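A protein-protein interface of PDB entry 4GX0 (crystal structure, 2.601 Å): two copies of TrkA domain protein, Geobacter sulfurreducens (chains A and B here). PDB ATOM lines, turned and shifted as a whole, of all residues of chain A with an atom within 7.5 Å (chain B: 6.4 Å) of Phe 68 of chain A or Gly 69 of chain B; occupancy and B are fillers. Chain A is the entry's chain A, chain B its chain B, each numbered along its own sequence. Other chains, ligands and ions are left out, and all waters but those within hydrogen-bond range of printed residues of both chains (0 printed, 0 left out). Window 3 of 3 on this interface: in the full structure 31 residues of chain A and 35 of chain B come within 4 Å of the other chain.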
ATOM      1  N   TYR A  57     -23.726  -6.794 -21.110  1.00  0.00           N
ATOM      2  CA  TYR A  57     -23.709  -6.108 -19.821  1.00  0.00           C
ATOM      3  C   TYR A  57     -22.327  -5.562 -19.471  1.00  0.00           C
ATOM      4  O   TYR A  57     -22.200  -4.451 -18.951  1.00  0.00           O
ATOM      5  CB  TYR A  57     -24.211  -7.066 -18.741  1.00  0.00           C
ATOM      6  CG  TYR A  57     -23.827  -6.732 -17.318  1.00  0.00           C
ATOM      7  CD1 TYR A  57     -24.536  -5.788 -16.586  1.00  0.00           C
ATOM      8  CD2 TYR A  57     -22.783  -7.399 -16.690  1.00  0.00           C
ATOM      9  CE1 TYR A  57     -24.197  -5.501 -15.275  1.00  0.00           C
ATOM     10  CE2 TYR A  57     -22.436  -7.120 -15.384  1.00  0.00           C
ATOM     11  CZ  TYR A  57     -23.145  -6.173 -14.680  1.00  0.00           C
ATOM     12  OH  TYR A  57     -22.800  -5.899 -13.378  1.00  0.00           O
ATOM     13  N   THR A  61     -21.161  -1.678 -19.588  1.00  0.00           N
ATOM     14  CA  THR A  61     -20.582  -1.236 -18.321  1.00  0.00           C
ATOM     15  C   THR A  61     -19.243  -0.524 -18.508  1.00  0.00           C
ATOM     16  O   THR A  61     -18.926   0.422 -17.783  1.00  0.00           O
ATOM     17  CB  THR A  61     -20.408  -2.423 -17.345  1.00  0.00           C
ATOM     18  OG1 THR A  61     -21.664  -2.711 -16.720  1.00  0.00           O
ATOM     19  CG2 THR A  61     -19.376  -2.105 -16.271  1.00  0.00           C
ATOM     20  N   VAL A  62     -18.465  -0.981 -19.485  1.00  0.00           N
ATOM     21  CA  VAL A  62     -17.159  -0.395 -19.767  1.00  0.00           C
ATOM     22  C   VAL A  62     -17.253   0.876 -20.615  1.00  0.00           C
ATOM     23  O   VAL A  62     -16.687   1.907 -20.256  1.00  0.00           O
ATOM     24  CB  VAL A  62     -16.226  -1.397 -20.472  1.00  0.00           C
ATOM     25  CG1 VAL A  62     -14.965  -0.698 -20.940  1.00  0.00           C
ATOM     26  CG2 VAL A  62     -15.887  -2.556 -19.543  1.00  0.00           C
ATOM     27  N   THR A  65     -18.627   3.727 -19.129  1.00  0.00           N
ATOM     28  CA  THR A  65     -17.732   4.098 -18.042  1.00  0.00           C
ATOM     29  C   THR A  65     -18.301   3.877 -16.677  1.00  0.00           C
ATOM     30  O   THR A  65     -17.809   4.414 -15.754  1.00  0.00           O
ATOM     31  CB  THR A  65     -17.243   5.520 -18.094  1.00  0.00           C
ATOM     32  OG1 THR A  65     -18.279   6.342 -18.609  1.00  0.00           O
ATOM     33  CG2 THR A  65     -16.054   5.635 -18.975  1.00  0.00           C
ATOM     34  N   LEU A  66     -19.340   3.084 -16.552  1.00  0.00           N
ATOM     35  CA  LEU A  66     -19.913   2.846 -15.254  1.00  0.00           C
ATOM     36  C   LEU A  66     -18.806   2.210 -14.495  1.00  0.00           C
ATOM     37  O   LEU A  66     -18.301   2.746 -13.556  1.00  0.00           O
ATOM     38  CB  LEU A  66     -21.071   1.895 -15.368  1.00  0.00           C
ATOM     39  CG  LEU A  66     -22.146   2.035 -14.322  1.00  0.00           C
ATOM     40  CD1 LEU A  66     -22.837   0.780 -14.242  1.00  0.00           C
ATOM     41  CD2 LEU A  66     -21.555   2.313 -13.042  1.00  0.00           C
ATOM     42  N   GLY A  67     -18.420   1.040 -14.936  1.00  0.00           N
ATOM     43  CA  GLY A  67     -17.330   0.292 -14.327  1.00  0.00           C
ATOM     44  C   GLY A  67     -17.583  -0.482 -13.037  1.00  0.00           C
ATOM     45  O   GLY A  67     -16.766  -0.425 -12.133  1.00  0.00           O
ATOM     46  N   PHE A  68     -18.620  -1.282 -12.977  1.00  0.00           N
ATOM     47  CA  PHE A  68     -18.900  -2.078 -11.804  1.00  0.00           C
ATOM     48  C   PHE A  68     -17.720  -2.867 -11.256  1.00  0.00           C
ATOM     49  O   PHE A  68     -17.566  -3.000 -10.077  1.00  0.00           O
ATOM     50  CB  PHE A  68     -20.009  -3.042 -12.109  1.00  0.00           C
ATOM     51  CG  PHE A  68     -21.346  -2.478 -11.933  1.00  0.00           C
ATOM     52  CD1 PHE A  68     -22.360  -2.829 -12.754  1.00  0.00           C
ATOM     53  CD2 PHE A  68     -21.597  -1.600 -10.947  1.00  0.00           C
ATOM     54  CE1 PHE A  68     -23.587  -2.315 -12.570  1.00  0.00           C
ATOM     55  CE2 PHE A  68     -22.811  -1.100 -10.769  1.00  0.00           C
ATOM     56  CZ  PHE A  68     -23.803  -1.449 -11.571  1.00  0.00           C
ATOM     57  N   GLY A  69     -16.889  -3.409 -12.118  1.00  0.00           N
ATOM     58  CA  GLY A  69     -15.741  -4.174 -11.684  1.00  0.00           C
ATOM     59  C   GLY A  69     -15.991  -5.589 -11.247  1.00  0.00           C
ATOM     60  O   GLY A  69     -15.099  -6.259 -10.815  1.00  0.00           O
ATOM     61  N   ASP A  70     -17.240  -6.034 -11.329  1.00  0.00           N
ATOM     62  CA  ASP A  70     -17.589  -7.391 -10.924  1.00  0.00           C
ATOM     63  C   ASP A  70     -17.032  -8.410 -11.909  1.00  0.00           C
ATOM     64  O   ASP A  70     -16.912  -9.591 -11.585  1.00  0.00           O
ATOM     65  CB  ASP A  70     -19.107  -7.550 -10.797  1.00  0.00           C
ATOM     66  CG  ASP A  70     -19.851  -7.088 -12.042  1.00  0.00           C
ATOM     67  OD1 ASP A  70     -19.255  -6.350 -12.857  1.00  0.00           O
ATOM     68  OD2 ASP A  70     -21.036  -7.454 -12.198  1.00  0.00           O
ATOM     69  N   ILE A  71     -16.696  -7.942 -13.108  1.00  0.00           N
ATOM     70  CA  ILE A  71     -16.112  -8.794 -14.138  1.00  0.00           C
ATOM     71  C   ILE A  71     -14.891  -8.133 -14.769  1.00  0.00           C
ATOM     72  O   ILE A  71     -15.022  -7.248 -15.615  1.00  0.00           O
ATOM     73  CB  ILE A  71     -17.131  -9.122 -15.238  1.00  0.00           C
ATOM     74  CG1 ILE A  71     -18.385  -9.749 -14.630  1.00  0.00           C
ATOM     75  CG2 ILE A  71     -16.517 -10.051 -16.273  1.00  0.00           C
ATOM     76  CD1 ILE A  71     -19.476 -10.023 -15.639  1.00  0.00           C
ATOM     77  N   THR A  72     -13.706  -8.566 -14.350  1.00  0.00           N
ATOM     78  CA  THR A  72     -12.454  -8.030 -14.871  1.00  0.00           C
ATOM     79  C   THR A  72     -11.553  -9.159 -15.356  1.00  0.00           C
ATOM     80  O   THR A  72     -11.656 -10.289 -14.880  1.00  0.00           O
ATOM     81  CB  THR A  72     -11.694  -7.223 -13.795  1.00  0.00           C
ATOM     82  OG1 THR A  72     -11.417  -8.065 -12.670  1.00  0.00           O
ATOM     83  CG2 THR A  72     -12.520  -6.027 -13.332  1.00  0.00           C
ATOM     84  N   TRP B  58     -28.223   2.159  -4.738  1.00  0.00           N
ATOM     85  CA  TRP B  58     -27.803   1.445  -5.941  1.00  0.00           C
ATOM     86  C   TRP B  58     -28.201   2.197  -7.213  1.00  0.00           C
ATOM     87  O   TRP B  58     -27.372   2.432  -8.093  1.00  0.00           O
ATOM     88  CB  TRP B  58     -28.395   0.032  -5.963  1.00  0.00           C
ATOM     89  CG  TRP B  58     -28.053  -0.757  -7.198  1.00  0.00           C
ATOM     90  CD1 TRP B  58     -26.948  -1.531  -7.397  1.00  0.00           C
ATOM     91  CD2 TRP B  58     -28.829  -0.852  -8.402  1.00  0.00           C
ATOM     92  NE1 TRP B  58     -26.984  -2.101  -8.645  1.00  0.00           N
ATOM     93  CE2 TRP B  58     -28.129  -1.701  -9.283  1.00  0.00           C
ATOM     94  CE3 TRP B  58     -30.044  -0.299  -8.821  1.00  0.00           C
ATOM     95  CZ2 TRP B  58     -28.601  -2.010 -10.558  1.00  0.00           C
ATOM     96  CZ3 TRP B  58     -30.512  -0.606 -10.090  1.00  0.00           C
ATOM     97  CH2 TRP B  58     -29.792  -1.453 -10.942  1.00  0.00           C
ATOM     98  N   THR B  61     -26.289   5.167  -7.800  1.00  0.00           N
ATOM     99  CA  THR B  61     -24.935   4.709  -8.103  1.00  0.00           C
ATOM    100  C   THR B  61     -24.761   4.313  -9.572  1.00  0.00           C
ATOM    101  O   THR B  61     -23.677   4.458 -10.138  1.00  0.00           O
ATOM    102  CB  THR B  61     -24.533   3.526  -7.187  1.00  0.00           C
ATOM    103  OG1 THR B  61     -24.248   4.017  -5.872  1.00  0.00           O
ATOM    104  CG2 THR B  61     -23.307   2.804  -7.729  1.00  0.00           C
ATOM    105  N   VAL B  62     -25.830   3.818 -10.186  1.00  0.00           N
ATOM    106  CA  VAL B  62     -25.771   3.377 -11.575  1.00  0.00           C
ATOM    107  C   VAL B  62     -26.111   4.501 -12.556  1.00  0.00           C
ATOM    108  O   VAL B  62     -25.336   4.792 -13.471  1.00  0.00           O
ATOM    109  CB  VAL B  62     -26.712   2.185 -11.829  1.00  0.00           C
ATOM    110  CG1 VAL B  62     -26.689   1.798 -13.294  1.00  0.00           C
ATOM    111  CG2 VAL B  62     -26.321   0.998 -10.949  1.00  0.00           C
ATOM    112  N   LEU B  66     -21.450   6.002 -11.155  1.00  0.00           N
ATOM    113  CA  LEU B  66     -20.396   5.907 -10.171  1.00  0.00           C
ATOM    114  C   LEU B  66     -19.965   4.476 -10.251  1.00  0.00           C
ATOM    115  O   LEU B  66     -18.849   4.166 -10.526  1.00  0.00           O
ATOM    116  CB  LEU B  66     -20.967   6.276  -8.819  1.00  0.00           C
ATOM    117  CG  LEU B  66     -20.146   6.701  -7.622  1.00  0.00           C
ATOM    118  CD1 LEU B  66     -20.424   5.805  -6.528  1.00  0.00           C
ATOM    119  CD2 LEU B  66     -18.735   6.779  -7.891  1.00  0.00           C
ATOM    120  N   GLY B  67     -20.890   3.592 -10.009  1.00  0.00           N
ATOM    121  CA  GLY B  67     -20.660   2.158 -10.106  1.00  0.00           C
ATOM    122  C   GLY B  67     -19.680   1.526  -9.127  1.00  0.00           C
ATOM    123  O   GLY B  67     -18.710   0.921  -9.552  1.00  0.00           O
ATOM    124  N   PHE B  68     -19.980   1.631  -7.852  1.00  0.00           N
ATOM    125  CA  PHE B  68     -19.159   1.054  -6.828  1.00  0.00           C
ATOM    126  C   PHE B  68     -18.913  -0.421  -7.062  1.00  0.00           C
ATOM    127  O   PHE B  68     -17.813  -0.877  -6.963  1.00  0.00           O
ATOM    128  CB  PHE B  68     -19.840   1.221  -5.499  1.00  0.00           C
ATOM    129  CG  PHE B  68     -19.559   2.494  -4.854  1.00  0.00           C
ATOM    130  CD1 PHE B  68     -20.550   3.238  -4.327  1.00  0.00           C
ATOM    131  CD2 PHE B  68     -18.300   2.954  -4.779  1.00  0.00           C
ATOM    132  CE1 PHE B  68     -20.276   4.398  -3.738  1.00  0.00           C
ATOM    133  CE2 PHE B  68     -18.033   4.102  -4.199  1.00  0.00           C
ATOM    134  CZ  PHE B  68     -19.013   4.826  -3.671  1.00  0.00           C
ATOM    135  N   GLY B  69     -19.944  -1.172  -7.372  1.00  0.00           N
ATOM    136  CA  GLY B  69     -19.784  -2.575  -7.613  1.00  0.00           C
ATOM    137  C   GLY B  69     -19.974  -3.439  -6.406  1.00  0.00           C
ATOM    138  O   GLY B  69     -19.822  -4.622  -6.499  1.00  0.00           O
ATOM    139  N   ASP B  70     -20.260  -2.837  -5.256  1.00  0.00           N
ATOM    140  CA  ASP B  70     -20.467  -3.607  -4.031  1.00  0.00           C
ATOM    141  C   ASP B  70     -21.799  -4.347  -4.083  1.00  0.00           C
ATOM    142  O   ASP B  70     -21.995  -5.339  -3.390  1.00  0.00           O
ATOM    143  CB  ASP B  70     -20.397  -2.706  -2.790  1.00  0.00           C
ATOM    144  CG  ASP B  70     -21.357  -1.521  -2.867  1.00  0.00           C
ATOM    145  OD1 ASP B  70     -21.646  -1.053  -3.992  1.00  0.00           O
ATOM    146  OD2 ASP B  70     -21.819  -1.054  -1.799  1.00  0.00           O
ATOM    147  N   ILE B  71     -22.715  -3.850  -4.907  1.00  0.00           N
ATOM    148  CA  ILE B  71     -23.993  -4.511  -5.128  1.00  0.00           C
ATOM    149  C   ILE B  71     -24.222  -4.722  -6.621  1.00  0.00           C
ATOM    150  O   ILE B  71     -24.506  -3.776  -7.355  1.00  0.00           O
ATOM    151  CB  ILE B  71     -25.161  -3.690  -4.561  1.00  0.00           C
ATOM    152  CG1 ILE B  71     -24.941  -3.399  -3.076  1.00  0.00           C
ATOM    153  CG2 ILE B  71     -26.475  -4.421  -4.777  1.00  0.00           C
ATOM    154  CD1 ILE B  71     -26.038  -2.560  -2.457  1.00  0.00           C
ATOM    155  N   THR B  72     -24.090  -5.966  -7.065  1.00  0.00           N
ATOM    156  CA  THR B  72     -24.293  -6.305  -8.468  1.00  0.00           C
ATOM    157  C   THR B  72     -25.152  -7.557  -8.576  1.00  0.00           C
ATOM    158  O   THR B  72     -25.253  -8.323  -7.624  1.00  0.00           O
ATOM    159  CB  THR B  72     -22.952  -6.552  -9.194  1.00  0.00           C
ATOM    160  OG1 THR B  72     -22.271  -7.654  -8.583  1.00  0.00           O
ATOM    161  CG2 THR B  72     -22.066  -5.323  -9.118  1.00  0.00           C
ATOM    162  N   ALA B  82     -29.702  -4.091 -15.065  1.00  0.00           N
ATOM    163  CA  ALA B  82     -28.618  -3.172 -14.745  1.00  0.00           C
ATOM    164  C   ALA B  82     -28.196  -2.414 -15.993  1.00  0.00           C
ATOM    165  O   ALA B  82     -27.870  -1.230 -15.929  1.00  0.00           O
ATOM    166  CB  ALA B  82     -27.431  -3.921 -14.156  1.00  0.00           C
ATOM    167  N   THR B  86     -28.434   1.591 -16.535  1.00  0.00           N
ATOM    168  CA  THR B  86     -27.191   2.258 -16.904  1.00  0.00           C
ATOM    169  C   THR B  86     -27.390   3.191 -18.095  1.00  0.00           C
ATOM    170  O   THR B  86     -26.999   4.360 -18.059  1.00  0.00           O
ATOM    171  CB  THR B  86     -26.091   1.238 -17.232  1.00  0.00           C
ATOM    172  OG1 THR B  86     -25.638   0.627 -16.019  1.00  0.00           O
ATOM    173  CG2 THR B  86     -24.914   1.919 -17.917  1.00  0.00           C
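O of Leu 66 of chain A sits close to O of Leu 66 of chain B (3.4 Å).
The backbone carbonyl oxygen (O) of Tyr 57 of chain A lies within hydrogen-bond range of the side-chain hydroxyl (OG1) of Thr 61 of chain A, at 2.9 Å. OD2 of Asp 70 of chain A sits at hydrogen-bond distance from OH of Tyr 57 of chain A (2.6 Å). The backbone NH of Leu 66 of chain A sits at hydrogen-bond distance from the backbone carbonyl oxygen of Thr 61 of chain A. The backbone carbonyl oxygen of Thr 61 of chain A lies within hydrogen-bond range of the backbone NH of Gly 67 of chain A. The backbone carbonyl oxygen (O) of Thr 61 of chain B sits at hydrogen-bond distance from the backbone NH (N) of Leu 66 of chain B, at 2.9 Å. The backbone carbonyl oxygen (O) of Ala 82 of chain B sits at hydrogen-bond distance from the side-chain hydroxyl (OG1) of Thr 86 of chain B (2.9 Å).
Among the printed residues, pairs that only touch across the chains: Tyr 57 of chain A with Ala 82 of chain B, Leu 66 of chain A with Gly 67 of chain B, Leu 66 of chain A with Thr 86 of chain B, Gly 67 of chain A with Gly 67 of chain B, Phe 68 of chain A with Val 62 of chain B, Phe 68 of chain A with Gly 67 of chain B, Phe 68 of chain A with Phe 68 of chain B, Phe 68 of chain A with Gly 69 of chain B and Asp 70 of chain A with Thr 72 of chain B.
Printed residues of chain A within 4 Å of Gly 69 of chain B: Phe 68 (3.3 Å). Of the printed residues of chain A, Thr 72 of chain B touches Asp 70. Of the printed residues of chain B, Leu 66 of chain A touches Leu 66, Gly 67 and Thr 86. Of the printed residues of chain B, Asp 70 of chain A touches Thr 72 (3.7 Å). Ile 71 of chain A touches none of the printed residues of chain B. Trp 58 of chain B touches none of the printed residues of chain A. The nearest residue of chain B that does not touch Phe 68 of chain A is Thr 72 of chain B (4.1 Å). The nearest residue of chain A that does not touch Gly 69 of chain B is Asp 70 of chain A (5.2 Å). The nearest printed residue of chain A that does not touch Val 62 of chain B is Leu 66 of chain A (4.1 Å).
Of the 12 printed residues of chain B, 8 touch a printed residue of chain A. Of the 11 printed residues of chain A, 5 touch a printed residue of chain B. Hydrophobic or aromatic side chains of chain A that line the printed part of chain B: Tyr 57, Leu 66 and Phe 68. Along chain A the printed residues that touch a printed residue of chain B span positions 57 to 70. Among the printed residues, no Asp or Glu carboxylate lies within 4 Å of a Lys or Arg side-chain nitrogen of the other chain.
Gly 67 of chain B touches its own counterpart, Gly 67 of chain A. Phe 68 of chain A touches Gly 67 of chain B, but with the chains exchanged Gly 67 of chain A does not touch Phe 68 of chain B (5.3 Å). Phe 68 of chain A touches its own counterpart, Phe 68 of chain B. Phe 68 of chain A touches Gly 69 of chain B, but with the chains exchanged Gly 69 of chain A does not touch Phe 68 of chain B (5.8 Å).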
